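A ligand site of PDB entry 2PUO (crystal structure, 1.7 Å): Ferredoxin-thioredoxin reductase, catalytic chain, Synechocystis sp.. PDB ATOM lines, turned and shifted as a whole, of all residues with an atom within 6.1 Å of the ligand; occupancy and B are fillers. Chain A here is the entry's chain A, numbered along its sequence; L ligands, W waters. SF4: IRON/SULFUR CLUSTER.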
ATOM      1  N   PHE A  11       1.376  31.526   7.417  1.00  0.00           N
ATOM      2  CA  PHE A  11       1.233  30.492   6.396  1.00  0.00           C
ATOM      3  C   PHE A  11       2.594  29.987   5.928  1.00  0.00           C
ATOM      4  O   PHE A  11       2.818  28.773   5.845  1.00  0.00           O
ATOM      5  CB  PHE A  11       0.483  31.034   5.180  1.00  0.00           C
ATOM      6  CG  PHE A  11       0.828  30.310   3.902  1.00  0.00           C
ATOM      7  CD1 PHE A  11       0.455  28.980   3.708  1.00  0.00           C
ATOM      8  CD2 PHE A  11       1.623  30.934   2.939  1.00  0.00           C
ATOM      9  CE1 PHE A  11       0.884  28.276   2.581  1.00  0.00           C
ATOM     10  CE2 PHE A  11       2.056  30.237   1.807  1.00  0.00           C
ATOM     11  CZ  PHE A  11       1.681  28.897   1.635  1.00  0.00           C
ATOM     12  N   TYR A  15       3.937  26.256   6.458  1.00  0.00           N
ATOM     13  CA  TYR A  15       4.105  25.434   5.265  1.00  0.00           C
ATOM     14  C   TYR A  15       5.551  24.935   5.171  1.00  0.00           C
ATOM     15  O   TYR A  15       5.791  23.787   4.778  1.00  0.00           O
ATOM     16  CB  TYR A  15       3.759  26.222   3.994  1.00  0.00           C
ATOM     17  CG  TYR A  15       3.633  25.315   2.787  1.00  0.00           C
ATOM     18  CD1 TYR A  15       2.590  24.395   2.684  1.00  0.00           C
ATOM     19  CD2 TYR A  15       4.581  25.350   1.760  1.00  0.00           C
ATOM     20  CE1 TYR A  15       2.494  23.514   1.601  1.00  0.00           C
ATOM     21  CE2 TYR A  15       4.489  24.478   0.673  1.00  0.00           C
ATOM     22  CZ  TYR A  15       3.442  23.566   0.601  1.00  0.00           C
ATOM     23  OH  TYR A  15       3.362  22.689  -0.465  1.00  0.00           O
ATOM     24  N   VAL A  33       9.033  38.212  -0.809  1.00  0.00           N
ATOM     25  CA  VAL A  33       8.030  37.302  -1.357  1.00  0.00           C
ATOM     26  C   VAL A  33       6.755  37.286  -0.503  1.00  0.00           C
ATOM     27  O   VAL A  33       5.644  37.354  -1.030  1.00  0.00           O
ATOM     28  CB  VAL A  33       8.578  35.863  -1.466  1.00  0.00           C
ATOM     29  CG1 VAL A  33       7.481  34.925  -1.963  1.00  0.00           C
ATOM     30  CG2 VAL A  33       9.779  35.833  -2.407  1.00  0.00           C
ATOM     31  N   LEU A  37       3.036  38.213  -1.632  1.00  0.00           N
ATOM     32  CA  LEU A  37       1.912  37.291  -1.527  1.00  0.00           C
ATOM     33  C   LEU A  37       0.745  37.973  -0.840  1.00  0.00           C
ATOM     34  O   LEU A  37      -0.400  37.891  -1.290  1.00  0.00           O
ATOM     35  CB  LEU A  37       2.329  36.045  -0.736  1.00  0.00           C
ATOM     36  CG  LEU A  37       3.179  35.016  -1.495  1.00  0.00           C
ATOM     37  CD1 LEU A  37       3.721  33.964  -0.525  1.00  0.00           C
ATOM     38  CD2 LEU A  37       2.329  34.360  -2.564  1.00  0.00           C
ATOM     39  N   PRO A  47      -3.457  34.385  -2.854  1.00  0.00           N
ATOM     40  CA  PRO A  47      -2.022  34.671  -2.831  1.00  0.00           C
ATOM     41  C   PRO A  47      -1.318  34.272  -4.125  1.00  0.00           C
ATOM     42  O   PRO A  47      -0.458  33.392  -4.144  1.00  0.00           O
ATOM     43  CB  PRO A  47      -1.542  33.858  -1.633  1.00  0.00           C
ATOM     44  CG  PRO A  47      -2.426  32.662  -1.671  1.00  0.00           C
ATOM     45  CD  PRO A  47      -3.790  33.261  -1.969  1.00  0.00           C
ATOM     46  N   LEU A  48      -1.687  34.927  -5.221  1.00  0.00           N
ATOM     47  CA  LEU A  48      -1.070  34.639  -6.516  1.00  0.00           C
ATOM     48  C   LEU A  48       0.430  34.858  -6.414  1.00  0.00           C
ATOM     49  O   LEU A  48       0.876  35.846  -5.833  1.00  0.00           O
ATOM     50  CB  LEU A  48      -1.659  35.552  -7.583  1.00  0.00           C
ATOM     51  CG  LEU A  48      -1.184  35.332  -9.028  1.00  0.00           C
ATOM     52  CD1 LEU A  48      -1.476  33.901  -9.456  1.00  0.00           C
ATOM     53  CD2 LEU A  48      -1.904  36.314  -9.949  1.00  0.00           C
ATOM     54  N   CYS A  49       1.215  33.944  -6.969  1.00  0.00           N
ATOM     55  CA  CYS A  49       2.662  34.080  -6.917  1.00  0.00           C
ATOM     56  C   CYS A  49       3.068  35.493  -7.360  1.00  0.00           C
ATOM     57  O   CYS A  49       2.660  35.948  -8.423  1.00  0.00           O
ATOM     58  CB  CYS A  49       3.352  33.051  -7.807  1.00  0.00           C
ATOM     59  SG  CYS A  49       5.139  33.129  -7.638  1.00  0.00           S
ATOM     60  N   PRO A  50       3.880  36.184  -6.547  1.00  0.00           N
ATOM     61  CA  PRO A  50       4.342  37.553  -6.840  1.00  0.00           C
ATOM     62  C   PRO A  50       5.550  37.711  -7.752  1.00  0.00           C
ATOM     63  O   PRO A  50       5.840  38.827  -8.211  1.00  0.00           O
ATOM     64  CB  PRO A  50       4.629  38.105  -5.452  1.00  0.00           C
ATOM     65  CG  PRO A  50       5.213  36.902  -4.760  1.00  0.00           C
ATOM     66  CD  PRO A  50       4.259  35.788  -5.182  1.00  0.00           C
ATOM     67  N   CYS A  51       6.259  36.621  -8.014  1.00  0.00           N
ATOM     68  CA  CYS A  51       7.440  36.704  -8.865  1.00  0.00           C
ATOM     69  C   CYS A  51       7.187  36.246 -10.300  1.00  0.00           C
ATOM     70  O   CYS A  51       8.024  35.578 -10.905  1.00  0.00           O
ATOM     71  CB  CYS A  51       8.573  35.890  -8.241  1.00  0.00           C
ATOM     72  SG  CYS A  51       9.154  36.529  -6.631  1.00  0.00           S
ATOM     73  N   TRP A  66      -1.115  29.057 -10.037  1.00  0.00           N
ATOM     74  CA  TRP A  66      -0.082  29.862  -9.396  1.00  0.00           C
ATOM     75  C   TRP A  66      -0.428  30.437  -8.015  1.00  0.00           C
ATOM     76  O   TRP A  66       0.305  31.288  -7.504  1.00  0.00           O
ATOM     77  CB  TRP A  66       0.364  30.999 -10.326  1.00  0.00           C
ATOM     78  CG  TRP A  66       1.229  30.542 -11.483  1.00  0.00           C
ATOM     79  CD1 TRP A  66       0.972  30.684 -12.813  1.00  0.00           C
ATOM     80  CD2 TRP A  66       2.494  29.874 -11.385  1.00  0.00           C
ATOM     81  NE1 TRP A  66       1.992  30.144 -13.552  1.00  0.00           N
ATOM     82  CE2 TRP A  66       2.941  29.639 -12.710  1.00  0.00           C
ATOM     83  CE3 TRP A  66       3.299  29.453 -10.321  1.00  0.00           C
ATOM     84  CZ2 TRP A  66       4.161  28.995 -12.993  1.00  0.00           C
ATOM     85  CZ3 TRP A  66       4.506  28.816 -10.601  1.00  0.00           C
ATOM     86  CH2 TRP A  66       4.921  28.595 -11.924  1.00  0.00           C
ATOM     87  N   ASN A  67      -1.522  29.984  -7.426  1.00  0.00           N
ATOM     88  CA  ASN A  67      -1.878  30.461  -6.093  1.00  0.00           C
ATOM     89  C   ASN A  67      -0.996  29.713  -5.103  1.00  0.00           C
ATOM     90  O   ASN A  67      -0.974  28.477  -5.077  1.00  0.00           O
ATOM     91  CB  ASN A  67      -3.356  30.188  -5.798  1.00  0.00           C
ATOM     92  CG  ASN A  67      -4.284  31.117  -6.562  1.00  0.00           C
ATOM     93  OD1 ASN A  67      -3.854  32.170  -7.048  1.00  0.00           O
ATOM     94  ND2 ASN A  67      -5.550  30.760  -6.648  1.00  0.00           N
ATOM     95  N   CYS A  68      -0.262  30.455  -4.280  1.00  0.00           N
ATOM     96  CA  CYS A  68       0.661  29.862  -3.315  1.00  0.00           C
ATOM     97  C   CYS A  68      -0.016  29.026  -2.233  1.00  0.00           C
ATOM     98  O   CYS A  68      -0.968  29.470  -1.606  1.00  0.00           O
ATOM     99  CB  CYS A  68       1.485  30.964  -2.656  1.00  0.00           C
ATOM    100  SG  CYS A  68       2.900  30.364  -1.712  1.00  0.00           S
ATOM    101  N   PRO A  69       0.484  27.796  -1.992  1.00  0.00           N
ATOM    102  CA  PRO A  69       1.623  27.164  -2.677  1.00  0.00           C
ATOM    103  C   PRO A  69       1.179  26.632  -4.038  1.00  0.00           C
ATOM    104  O   PRO A  69       0.195  25.895  -4.127  1.00  0.00           O
ATOM    105  CB  PRO A  69       2.040  26.059  -1.716  1.00  0.00           C
ATOM    106  CG  PRO A  69       0.729  25.630  -1.114  1.00  0.00           C
ATOM    107  CD  PRO A  69       0.039  26.958  -0.856  1.00  0.00           C
ATOM    108  N   CYS A  70       1.914  27.012  -5.073  1.00  0.00           N
ATOM    109  CA  CYS A  70       1.599  26.639  -6.453  1.00  0.00           C
ATOM    110  C   CYS A  70       1.779  25.160  -6.758  1.00  0.00           C
ATOM    111  O   CYS A  70       2.348  24.418  -5.952  1.00  0.00           O
ATOM    112  CB  CYS A  70       2.470  27.458  -7.389  1.00  0.00           C
ATOM    113  SG  CYS A  70       4.219  27.135  -7.191  1.00  0.00           S
ATOM    114  N   VAL A  71       1.309  24.744  -7.927  1.00  0.00           N
ATOM    115  CA  VAL A  71       1.392  23.354  -8.355  1.00  0.00           C
ATOM    116  C   VAL A  71       2.832  22.827  -8.375  1.00  0.00           C
ATOM    117  O   VAL A  71       3.086  21.715  -7.926  1.00  0.00           O
ATOM    118  CB  VAL A  71       0.753  23.160  -9.764  1.00  0.00           C
ATOM    119  CG1 VAL A  71       1.182  21.823 -10.359  1.00  0.00           C
ATOM    120  CG2 VAL A  71      -0.781  23.202  -9.644  1.00  0.00           C
ATOM    121  N   PRO A  72       3.784  23.619  -8.913  1.00  0.00           N
ATOM    122  CA  PRO A  72       5.175  23.149  -8.957  1.00  0.00           C
ATOM    123  C   PRO A  72       5.769  22.935  -7.554  1.00  0.00           C
ATOM    124  O   PRO A  72       6.659  22.102  -7.372  1.00  0.00           O
ATOM    125  CB  PRO A  72       5.902  24.247  -9.717  1.00  0.00           C
ATOM    126  CG  PRO A  72       4.826  24.767 -10.661  1.00  0.00           C
ATOM    127  CD  PRO A  72       3.620  24.834  -9.724  1.00  0.00           C
ATOM    128  N   MET A  73       5.300  23.698  -6.582  1.00  0.00           N
ATOM    129  CA  MET A  73       5.804  23.567  -5.227  1.00  0.00           C
ATOM    130  C   MET A  73       5.128  22.372  -4.571  1.00  0.00           C
ATOM    131  O   MET A  73       5.786  21.533  -3.945  1.00  0.00           O
ATOM    132  CB  MET A  73       5.509  24.814  -4.402  1.00  0.00           C
ATOM    133  CG  MET A  73       6.012  24.722  -2.944  1.00  0.00           C
ATOM    134  SD  MET A  73       7.790  24.454  -2.817  1.00  0.00           S
ATOM    135  CE  MET A  73       7.932  23.636  -1.207  1.00  0.00           C
ATOM    136  N   GLU A  78       9.208  22.760  -6.179  1.00  0.00           N
ATOM    137  CA  GLU A  78       9.935  23.757  -6.940  1.00  0.00           C
ATOM    138  C   GLU A  78       9.320  25.115  -6.622  1.00  0.00           C
ATOM    139  O   GLU A  78       8.142  25.359  -6.927  1.00  0.00           O
ATOM    140  CB  GLU A  78       9.854  23.452  -8.437  1.00  0.00           C
ATOM    141  CG  GLU A  78      10.439  22.086  -8.787  1.00  0.00           C
ATOM    142  CD  GLU A  78      10.461  21.827 -10.279  1.00  0.00           C
ATOM    143  OE1 GLU A  78       9.840  22.591 -11.043  1.00  0.00           O
ATOM    144  OE2 GLU A  78      11.116  20.837 -10.680  1.00  0.00           O
ATOM    145  N   CYS A  79      10.111  25.973  -6.000  1.00  0.00           N
ATOM    146  CA  CYS A  79       9.657  27.309  -5.627  1.00  0.00           C
ATOM    147  C   CYS A  79      10.508  28.368  -6.306  1.00  0.00           C
ATOM    148  O   CYS A  79      11.613  28.689  -5.857  1.00  0.00           O
ATOM    149  CB  CYS A  79       9.704  27.490  -4.113  1.00  0.00           C
ATOM    150  SG  CYS A  79       9.233  29.142  -3.541  1.00  0.00           S
ATOM    151  N   HIS A  80       9.981  28.884  -7.411  1.00  0.00           N
ATOM    152  CA  HIS A  80      10.632  29.899  -8.217  1.00  0.00           C
ATOM    153  C   HIS A  80      10.975  31.167  -7.430  1.00  0.00           C
ATOM    154  O   HIS A  80      12.017  31.781  -7.647  1.00  0.00           O
ATOM    155  CB  HIS A  80       9.719  30.216  -9.403  1.00  0.00           C
ATOM    156  CG  HIS A  80      10.055  31.489 -10.124  1.00  0.00           C
ATOM    157  ND1 HIS A  80       9.507  32.702  -9.773  1.00  0.00           N
ATOM    158  CD2 HIS A  80      10.853  31.728 -11.185  1.00  0.00           C
ATOM    159  CE1 HIS A  80       9.972  33.643 -10.583  1.00  0.00           C
ATOM    160  NE2 HIS A  80      10.785  33.069 -11.458  1.00  0.00           N
ATOM    161  N   CYS A  81      10.106  31.543  -6.491  1.00  0.00           N
ATOM    162  CA  CYS A  81      10.304  32.738  -5.678  1.00  0.00           C
ATOM    163  C   CYS A  81      11.436  32.641  -4.655  1.00  0.00           C
ATOM    164  O   CYS A  81      11.861  33.648  -4.097  1.00  0.00           O
ATOM    165  CB  CYS A  81       9.023  33.081  -4.933  1.00  0.00           C
ATOM    166  SG  CYS A  81       7.613  33.452  -5.963  1.00  0.00           S
ATOM    167  N   MET A  82      11.918  31.429  -4.396  1.00  0.00           N
ATOM    168  CA  MET A  82      12.969  31.226  -3.416  1.00  0.00           C
ATOM    169  C   MET A  82      12.444  31.461  -2.002  1.00  0.00           C
ATOM    170  O   MET A  82      13.148  31.988  -1.145  1.00  0.00           O
ATOM    171  CB  MET A  82      14.172  32.141  -3.682  1.00  0.00           C
ATOM    172  CG  MET A  82      15.038  31.695  -4.861  1.00  0.00           C
ATOM    173  SD  MET A  82      16.595  32.602  -4.938  1.00  0.00           S
ATOM    174  CE  MET A  82      17.406  31.970  -3.482  1.00  0.00           C
ATOM    175  N   LEU A  83      11.186  31.098  -1.788  1.00  0.00           N
ATOM    176  CA  LEU A  83      10.547  31.240  -0.482  1.00  0.00           C
ATOM    177  C   LEU A  83      10.757  29.942   0.307  1.00  0.00           C
ATOM    178  O   LEU A  83      11.216  29.961   1.448  1.00  0.00           O
ATOM    179  CB  LEU A  83       9.056  31.515  -0.645  1.00  0.00           C
ATOM    180  CG  LEU A  83       8.228  31.601   0.643  1.00  0.00           C
ATOM    181  CD1 LEU A  83       8.847  32.625   1.585  1.00  0.00           C
ATOM    182  CD2 LEU A  83       6.789  31.972   0.307  1.00  0.00           C
ATOM    183  N   PHE A  84      10.415  28.825  -0.332  1.00  0.00           N
ATOM    184  CA  PHE A  84      10.554  27.498   0.277  1.00  0.00           C
ATOM    185  C   PHE A  84      11.693  26.752  -0.412  1.00  0.00           C
ATOM    186  O   PHE A  84      11.570  26.355  -1.575  1.00  0.00           O
ATOM    187  CB  PHE A  84       9.262  26.695   0.115  1.00  0.00           C
ATOM    188  CG  PHE A  84       8.037  27.382   0.669  1.00  0.00           C
ATOM    189  CD1 PHE A  84       7.902  27.588   2.036  1.00  0.00           C
ATOM    190  CD2 PHE A  84       7.029  27.833  -0.181  1.00  0.00           C
ATOM    191  CE1 PHE A  84       6.779  28.236   2.555  1.00  0.00           C
ATOM    192  CE2 PHE A  84       5.901  28.490   0.329  1.00  0.00           C
ATOM    193  CZ  PHE A  84       5.783  28.694   1.705  1.00  0.00           C
HETATM  194 FE1  SF4 L   1       4.477  30.257  -3.479  1.00  0.00          FE
HETATM  195 FE2  SF4 L   1       4.953  28.934  -5.755  1.00  0.00          FE
HETATM  196 FE3  SF4 L   1       6.984  29.626  -4.185  1.00  0.00          FE
HETATM  197 FE4  SF4 L   1       5.700  31.543  -5.674  1.00  0.00          FE
HETATM  198  S1  SF4 L   1       6.983  29.808  -6.480  1.00  0.00           S
HETATM  199  S2  SF4 L   1       6.283  31.635  -3.450  1.00  0.00           S
HETATM  200  S3  SF4 L   1       3.656  30.765  -5.534  1.00  0.00           S
HETATM  201  S4  SF4 L   1       5.441  28.170  -3.675  1.00  0.00           S
HETATM  202  O   HOH W   1       7.270  27.230  -8.760  1.00  0.00           O
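Water W1 lies within hydrogen-bond range of the backbone carbonyl oxygen of Glu 78 (2.8 Å), the backbone NH of His 80 (3.5 Å) and a sulfur (S1) of the ligand (3.5 Å).
CG1 of Val 33 touches S2 of the ligand, 3.8 Å away.
Trp 66 touches the ligand.
CB of Met 73 touches S4 of the ligand, 3.4 Å away.
CD2 of Leu 83 touches S2 of the ligand (3.8 Å).
CD2 of Phe 84 touches S4 of the ligand, at 3.9 Å.
Hydrophobic or aromatic side chains within 4 Å of the ligand: Val 33, Met 73, Leu 83 and Phe 84.
Of the 24 residues printed, 11 come within 4 Å of the ligand.
The backbone NH (N) of Met 73 is in hydrogen-bond range of the backbone carbonyl oxygen (O) of Glu 78.
The backbone NH (N) of Cys 49 lies within hydrogen-bond range of the backbone carbonyl oxygen (O) of Trp 66, at 2.9 Å.
N of Phe 84 sits close to SG of Cys 79 (3.4 Å).
The side-chain sulfur of Cys 81 sits close to the side-chain sulfur of Cys 51, at 3.5 Å.
The side-chain sulfur (SG) of Cys 49 sits close to the backbone NH (N) of Cys 51 (3.7 Å).
N of Met 82 lies close to SG of Cys 79 (3.6 Å).
The side-chain sulfur (SG) of Cys 70 lies close to the backbone NH (N) of Met 73.
The backbone NH (N) of Cys 68 is in hydrogen-bond range of the backbone carbonyl oxygen (O) of Pro 47, 2.9 Å away.
FE4 of the ligand is bound by SG of Cys 49.
The side-chain sulfur of Cys 68 binds an iron atom (FE1) of the ligand, at 2.4 Å.
N of Cys 81 lies close to S1 of the ligand, 3.6 Å away.
The side-chain sulfur (SG) of Cys 70 is bound to an iron atom (FE2) of the ligand.
S1 of the ligand sits close to N of His 80 (3.3 Å).
The side-chain sulfur (SG) of Cys 79 binds an iron atom (FE3) of the ligand, at 2.4 Å.
SG of Cys 81 binds FE4 of the ligand, 2.7 Å away.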
